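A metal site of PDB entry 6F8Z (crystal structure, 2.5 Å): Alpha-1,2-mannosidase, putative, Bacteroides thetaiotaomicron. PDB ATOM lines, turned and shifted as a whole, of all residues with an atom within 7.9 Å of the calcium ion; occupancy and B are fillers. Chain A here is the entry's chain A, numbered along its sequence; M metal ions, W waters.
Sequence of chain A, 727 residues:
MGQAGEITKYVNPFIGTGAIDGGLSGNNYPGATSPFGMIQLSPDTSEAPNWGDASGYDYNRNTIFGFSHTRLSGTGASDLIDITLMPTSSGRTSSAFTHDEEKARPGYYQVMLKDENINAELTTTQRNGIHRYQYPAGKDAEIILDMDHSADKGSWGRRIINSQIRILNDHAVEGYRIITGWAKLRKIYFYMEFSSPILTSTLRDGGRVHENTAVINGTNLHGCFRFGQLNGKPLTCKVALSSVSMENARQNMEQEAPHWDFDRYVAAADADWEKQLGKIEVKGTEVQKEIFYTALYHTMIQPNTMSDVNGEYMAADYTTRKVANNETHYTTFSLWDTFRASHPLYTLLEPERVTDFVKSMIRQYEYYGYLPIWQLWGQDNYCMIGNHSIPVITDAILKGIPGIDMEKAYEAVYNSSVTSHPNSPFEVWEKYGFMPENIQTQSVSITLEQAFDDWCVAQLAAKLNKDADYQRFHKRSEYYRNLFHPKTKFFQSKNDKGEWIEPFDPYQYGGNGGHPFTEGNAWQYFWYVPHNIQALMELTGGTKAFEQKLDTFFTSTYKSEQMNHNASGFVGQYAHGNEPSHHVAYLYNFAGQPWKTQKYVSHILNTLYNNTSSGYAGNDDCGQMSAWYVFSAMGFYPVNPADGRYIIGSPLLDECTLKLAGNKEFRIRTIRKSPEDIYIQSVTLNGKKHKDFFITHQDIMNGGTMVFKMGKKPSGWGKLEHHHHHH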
ATOM      1  N   GLY A  74       7.523  11.706  -0.586  1.00  0.00           N
ATOM      2  CA  GLY A  74       8.709  11.293  -1.315  1.00  0.00           C
ATOM      3  C   GLY A  74       9.772  10.527  -0.558  1.00  0.00           C
ATOM      4  O   GLY A  74      10.918  10.470  -1.023  1.00  0.00           O
ATOM      5  N   GLY A  76      11.576   7.073   1.215  1.00  0.00           N
ATOM      6  CA  GLY A  76      11.790   5.656   0.866  1.00  0.00           C
ATOM      7  C   GLY A  76      11.311   4.679   1.931  1.00  0.00           C
ATOM      8  O   GLY A  76      11.558   3.484   1.802  1.00  0.00           O
ATOM      9  N   TRP A 336      19.746  14.375   5.123  1.00  0.00           N
ATOM     10  CA  TRP A 336      20.731  13.848   4.184  1.00  0.00           C
ATOM     11  C   TRP A 336      20.428  14.261   2.740  1.00  0.00           C
ATOM     12  O   TRP A 336      21.344  14.410   1.936  1.00  0.00           O
ATOM     13  CB  TRP A 336      20.828  12.328   4.277  1.00  0.00           C
ATOM     14  CG  TRP A 336      21.861  11.707   3.429  1.00  0.00           C
ATOM     15  CD1 TRP A 336      23.197  11.667   3.676  1.00  0.00           C
ATOM     16  CD2 TRP A 336      21.644  11.025   2.187  1.00  0.00           C
ATOM     17  NE1 TRP A 336      23.837  10.984   2.647  1.00  0.00           N
ATOM     18  CE2 TRP A 336      22.907  10.582   1.728  1.00  0.00           C
ATOM     19  CE3 TRP A 336      20.515  10.733   1.419  1.00  0.00           C
ATOM     20  CZ2 TRP A 336      23.057   9.865   0.540  1.00  0.00           C
ATOM     21  CZ3 TRP A 336      20.663  10.034   0.217  1.00  0.00           C
ATOM     22  CH2 TRP A 336      21.931   9.608  -0.203  1.00  0.00           C
ATOM     23  N   ASP A 337      19.146  14.447   2.425  1.00  0.00           N
ATOM     24  CA  ASP A 337      18.733  14.979   1.125  1.00  0.00           C
ATOM     25  C   ASP A 337      18.668  16.512   1.146  1.00  0.00           C
ATOM     26  O   ASP A 337      19.269  17.171   0.297  1.00  0.00           O
ATOM     27  CB  ASP A 337      17.377  14.428   0.681  1.00  0.00           C
ATOM     28  CG  ASP A 337      17.249  12.928   0.899  1.00  0.00           C
ATOM     29  OD1 ASP A 337      17.828  12.125   0.113  1.00  0.00           O
ATOM     30  OD2 ASP A 337      16.517  12.554   1.851  1.00  0.00           O
ATOM     31  N   MET A 384      20.250   7.319   7.012  1.00  0.00           N
ATOM     32  CA  MET A 384      21.374   7.783   6.197  1.00  0.00           C
ATOM     33  C   MET A 384      22.579   8.118   7.081  1.00  0.00           C
ATOM     34  O   MET A 384      22.820   7.398   8.042  1.00  0.00           O
ATOM     35  CB  MET A 384      20.961   8.914   5.229  1.00  0.00           C
ATOM     36  CG  MET A 384      19.679   8.635   4.443  1.00  0.00           C
ATOM     37  SD  MET A 384      19.631   7.020   3.632  1.00  0.00           S
ATOM     38  CE  MET A 384      21.097   7.109   2.624  1.00  0.00           C
ATOM     39  N   GLU A 519      24.131   3.929  -0.533  1.00  0.00           N
ATOM     40  CA  GLU A 519      23.243   3.987  -1.707  1.00  0.00           C
ATOM     41  C   GLU A 519      23.906   4.610  -2.925  1.00  0.00           C
ATOM     42  O   GLU A 519      23.404   5.554  -3.528  1.00  0.00           O
ATOM     43  CB  GLU A 519      21.926   4.708  -1.361  1.00  0.00           C
ATOM     44  CG  GLU A 519      21.029   3.988  -0.357  1.00  0.00           C
ATOM     45  CD  GLU A 519      19.784   4.770   0.003  1.00  0.00           C
ATOM     46  OE1 GLU A 519      19.491   5.818  -0.630  1.00  0.00           O
ATOM     47  OE2 GLU A 519      19.082   4.340   0.944  1.00  0.00           O
ATOM     48  N   ASN A 566      17.417   2.775  -5.211  1.00  0.00           N
ATOM     49  CA  ASN A 566      17.291   4.250  -5.074  1.00  0.00           C
ATOM     50  C   ASN A 566      17.992   5.042  -6.180  1.00  0.00           C
ATOM     51  O   ASN A 566      17.447   6.032  -6.700  1.00  0.00           O
ATOM     52  CB  ASN A 566      17.815   4.718  -3.711  1.00  0.00           C
ATOM     53  CG  ASN A 566      16.954   4.225  -2.549  1.00  0.00           C
ATOM     54  OD1 ASN A 566      15.793   4.615  -2.424  1.00  0.00           O
ATOM     55  ND2 ASN A 566      17.518   3.369  -1.705  1.00  0.00           N
ATOM     56  N   ALA A 567      19.213   4.621  -6.523  1.00  0.00           N
ATOM     57  CA  ALA A 567      19.972   5.222  -7.620  1.00  0.00           C
ATOM     58  C   ALA A 567      19.341   4.862  -8.973  1.00  0.00           C
ATOM     59  O   ALA A 567      19.330   3.690  -9.376  1.00  0.00           O
ATOM     60  CB  ALA A 567      21.425   4.761  -7.577  1.00  0.00           C
ATOM     61  N   SER A 568      18.802   5.885  -9.651  1.00  0.00           N
ATOM     62  CA  SER A 568      18.199   5.730 -10.985  1.00  0.00           C
ATOM     63  C   SER A 568      18.105   7.073 -11.745  1.00  0.00           C
ATOM     64  O   SER A 568      18.343   8.134 -11.158  1.00  0.00           O
ATOM     65  CB  SER A 568      16.828   5.075 -10.856  1.00  0.00           C
ATOM     66  N   ALA A 575      23.396   9.161 -11.680  1.00  0.00           N
ATOM     67  CA  ALA A 575      22.012   8.781 -11.374  1.00  0.00           C
ATOM     68  C   ALA A 575      21.323   9.952 -10.676  1.00  0.00           C
ATOM     69  O   ALA A 575      21.624  10.244  -9.517  1.00  0.00           O
ATOM     70  CB  ALA A 575      21.989   7.551 -10.483  1.00  0.00           C
ATOM     71  N   HIS A 576      20.388  10.582 -11.368  1.00  0.00           N
ATOM     72  CA  HIS A 576      19.712  11.733 -10.808  1.00  0.00           C
ATOM     73  C   HIS A 576      18.772  11.426  -9.626  1.00  0.00           C
ATOM     74  O   HIS A 576      18.451  12.344  -8.876  1.00  0.00           O
ATOM     75  CB  HIS A 576      18.962  12.525 -11.897  1.00  0.00           C
ATOM     76  CG  HIS A 576      18.615  13.916 -11.462  1.00  0.00           C
ATOM     77  ND1 HIS A 576      19.568  14.849 -11.136  1.00  0.00           N
ATOM     78  CD2 HIS A 576      17.418  14.499 -11.236  1.00  0.00           C
ATOM     79  CE1 HIS A 576      18.981  15.959 -10.732  1.00  0.00           C
ATOM     80  NE2 HIS A 576      17.674  15.774 -10.789  1.00  0.00           N
ATOM     81  N   GLY A 577      18.338  10.164  -9.454  1.00  0.00           N
ATOM     82  CA  GLY A 577      17.477   9.755  -8.312  1.00  0.00           C
ATOM     83  C   GLY A 577      18.123   9.722  -6.925  1.00  0.00           C
ATOM     84  O   GLY A 577      17.448   9.585  -5.832  1.00  0.00           O
ATOM     85  N   ASN A 578      19.444   9.829  -6.911  1.00  0.00           N
ATOM     86  CA  ASN A 578      20.077   9.870  -5.635  1.00  0.00           C
ATOM     87  C   ASN A 578      21.070  10.978  -5.507  1.00  0.00           C
ATOM     88  O   ASN A 578      21.887  11.224  -6.403  1.00  0.00           O
ATOM     89  CB  ASN A 578      20.606   8.482  -5.192  1.00  0.00           C
ATOM     90  CG  ASN A 578      20.030   8.023  -3.829  1.00  0.00           C
ATOM     91  OD1 ASN A 578      19.024   8.568  -3.347  1.00  0.00           O
ATOM     92  ND2 ASN A 578      20.660   7.034  -3.222  1.00  0.00           N
ATOM     93  N   GLU A 579      21.006  11.613  -4.352  1.00  0.00           N
ATOM     94  CA  GLU A 579      21.477  12.951  -4.211  1.00  0.00           C
ATOM     95  C   GLU A 579      22.976  13.135  -4.013  1.00  0.00           C
ATOM     96  O   GLU A 579      23.434  14.284  -4.003  1.00  0.00           O
ATOM     97  CB  GLU A 579      20.634  13.801  -3.225  1.00  0.00           C
ATOM     98  CG  GLU A 579      19.745  13.152  -2.203  1.00  0.00           C
ATOM     99  CD  GLU A 579      18.445  12.606  -2.741  1.00  0.00           C
ATOM    100  OE1 GLU A 579      17.421  13.307  -2.758  1.00  0.00           O
ATOM    101  OE2 GLU A 579      18.461  11.417  -3.065  1.00  0.00           O
ATOM    102  N   PRO A 580      23.757  12.034  -3.871  1.00  0.00           N
ATOM    103  CA  PRO A 580      25.190  12.306  -3.918  1.00  0.00           C
ATOM    104  C   PRO A 580      25.673  12.906  -5.266  1.00  0.00           C
ATOM    105  O   PRO A 580      26.551  13.751  -5.269  1.00  0.00           O
ATOM    106  CB  PRO A 580      25.810  10.929  -3.652  1.00  0.00           C
ATOM    107  CG  PRO A 580      24.813  10.266  -2.778  1.00  0.00           C
ATOM    108  CD  PRO A 580      23.485  10.679  -3.347  1.00  0.00           C
ATOM    109  N   HIS A 582      23.920  14.990  -7.199  1.00  0.00           N
ATOM    110  CA  HIS A 582      23.152  16.191  -7.581  1.00  0.00           C
ATOM    111  C   HIS A 582      23.909  17.471  -7.925  1.00  0.00           C
ATOM    112  O   HIS A 582      23.457  18.250  -8.746  1.00  0.00           O
ATOM    113  CB  HIS A 582      22.154  16.513  -6.466  1.00  0.00           C
ATOM    114  CG  HIS A 582      20.908  15.731  -6.560  1.00  0.00           C
ATOM    115  ND1 HIS A 582      19.800  16.016  -5.807  1.00  0.00           N
ATOM    116  CD2 HIS A 582      20.559  14.708  -7.371  1.00  0.00           C
ATOM    117  CE1 HIS A 582      18.820  15.185  -6.124  1.00  0.00           C
ATOM    118  NE2 HIS A 582      19.260  14.380  -7.075  1.00  0.00           N
ATOM    119  N   ALA A 617      12.936  11.296 -11.381  1.00  0.00           N
ATOM    120  CA  ALA A 617      13.855  10.200 -11.624  1.00  0.00           C
ATOM    121  C   ALA A 617      14.162   9.369 -10.362  1.00  0.00           C
ATOM    122  O   ALA A 617      15.197   8.715 -10.294  1.00  0.00           O
ATOM    123  CB  ALA A 617      15.152  10.753 -12.206  1.00  0.00           C
ATOM    124  N   GLY A 618      13.249   9.393  -9.389  1.00  0.00           N
ATOM    125  CA  GLY A 618      13.414   8.757  -8.103  1.00  0.00           C
ATOM    126  C   GLY A 618      12.548   9.466  -7.076  1.00  0.00           C
ATOM    127  O   GLY A 618      11.838  10.441  -7.388  1.00  0.00           O
ATOM    128  N   ASN A 619      12.604   8.978  -5.850  1.00  0.00           N
ATOM    129  CA  ASN A 619      11.871   9.572  -4.750  1.00  0.00           C
ATOM    130  C   ASN A 619      12.133  11.082  -4.585  1.00  0.00           C
ATOM    131  O   ASN A 619      13.266  11.533  -4.637  1.00  0.00           O
ATOM    132  CB  ASN A 619      12.220   8.850  -3.443  1.00  0.00           C
ATOM    133  CG  ASN A 619      11.644   7.421  -3.352  1.00  0.00           C
ATOM    134  OD1 ASN A 619      10.745   7.009  -4.102  1.00  0.00           O
ATOM    135  ND2 ASN A 619      12.173   6.682  -2.406  1.00  0.00           N
ATOM    136  N   ASP A 620      11.081  11.850  -4.347  1.00  0.00           N
ATOM    137  CA  ASP A 620      11.216  13.287  -4.245  1.00  0.00           C
ATOM    138  C   ASP A 620      12.026  13.730  -3.019  1.00  0.00           C
ATOM    139  O   ASP A 620      12.625  14.821  -3.021  1.00  0.00           O
ATOM    140  CB  ASP A 620       9.834  13.937  -4.264  1.00  0.00           C
ATOM    141  CG  ASP A 620       9.884  15.437  -4.515  1.00  0.00           C
ATOM    142  OD1 ASP A 620      10.847  15.938  -5.143  1.00  0.00           O
ATOM    143  OD2 ASP A 620       8.941  16.119  -4.074  1.00  0.00           O
ATOM    144  N   ASP A 621      12.047  12.885  -1.981  1.00  0.00           N
ATOM    145  CA  ASP A 621      12.889  13.059  -0.778  1.00  0.00           C
ATOM    146  C   ASP A 621      12.576  14.352  -0.059  1.00  0.00           C
ATOM    147  O   ASP A 621      13.441  15.213   0.108  1.00  0.00           O
ATOM    148  CB  ASP A 621      14.394  12.914  -1.113  1.00  0.00           C
ATOM    149  CG  ASP A 621      14.764  11.488  -1.508  1.00  0.00           C
ATOM    150  OD1 ASP A 621      14.271  10.579  -0.804  1.00  0.00           O
ATOM    151  OD2 ASP A 621      15.526  11.256  -2.491  1.00  0.00           O
ATOM    152  N   GLN A 624      13.536  17.419  -2.264  1.00  0.00           N
ATOM    153  CA  GLN A 624      14.917  17.678  -2.705  1.00  0.00           C
ATOM    154  C   GLN A 624      15.038  17.516  -4.218  1.00  0.00           C
ATOM    155  O   GLN A 624      15.738  18.292  -4.855  1.00  0.00           O
ATOM    156  CB  GLN A 624      15.920  16.780  -1.971  1.00  0.00           C
ATOM    157  CG  GLN A 624      17.351  16.805  -2.486  1.00  0.00           C
ATOM    158  CD  GLN A 624      17.990  18.192  -2.528  1.00  0.00           C
ATOM    159  OE1 GLN A 624      17.692  19.065  -1.711  1.00  0.00           O
ATOM    160  NE2 GLN A 624      18.891  18.381  -3.490  1.00  0.00           N
ATOM    161  N   MET A 625      14.363  16.521  -4.782  1.00  0.00           N
ATOM    162  CA  MET A 625      14.350  16.352  -6.255  1.00  0.00           C
ATOM    163  C   MET A 625      13.709  17.584  -6.926  1.00  0.00           C
ATOM    164  O   MET A 625      14.154  18.026  -7.983  1.00  0.00           O
ATOM    165  CB  MET A 625      13.594  15.075  -6.644  1.00  0.00           C
ATOM    166  CG  MET A 625      14.025  14.426  -7.953  1.00  0.00           C
ATOM    167  SD  MET A 625      15.560  13.472  -8.035  1.00  0.00           S
ATOM    168  CE  MET A 625      15.942  13.224  -6.317  1.00  0.00           C
HETATM  169 CA    CA M   1      16.983   9.678  -3.466  1.00  0.00          CA
HETATM  170  O   HOH W   1      17.025   9.455  -1.148  1.00  0.00           O
HETATM  171  O   HOH W   2      15.983   7.767  -2.669  1.00  0.00           O
HETATM  172  O   HOH W   3      15.465  10.372  -5.078  1.00  0.00           O
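The side-chain amide nitrogen of Asn 578 sits at hydrogen-bond distance from the side-chain carboxylate of Glu 519, at 3.1 Å. The backbone carbonyl oxygen (O) of Gly 74 is in hydrogen-bond range of the backbone NH (N) of Asp 621 (2.8 Å). The backbone NH (N) of Gly 577 is in hydrogen-bond range of the backbone carbonyl oxygen (O) of Ser 568, at 2.7 Å.
Water W2 binds the calcium ion, at 2.3 Å. The side-chain carboxylate (OE2) of Glu 579 binds the calcium ion. Water W3 binds the calcium ion. The side-chain amide oxygen (OD1) of Asn 578 binds the calcium ion. Water W1 binds the calcium ion. OD2 of Asp 621 is bound to the calcium ion. O of Gly 577 is bound to the calcium ion (2.4 Å).
Water W1 lies within hydrogen-bond range of the side-chain carboxylate of Asp 621 (3.0 Å) and the side-chain carboxylate of Asp 337 (3.1 Å).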
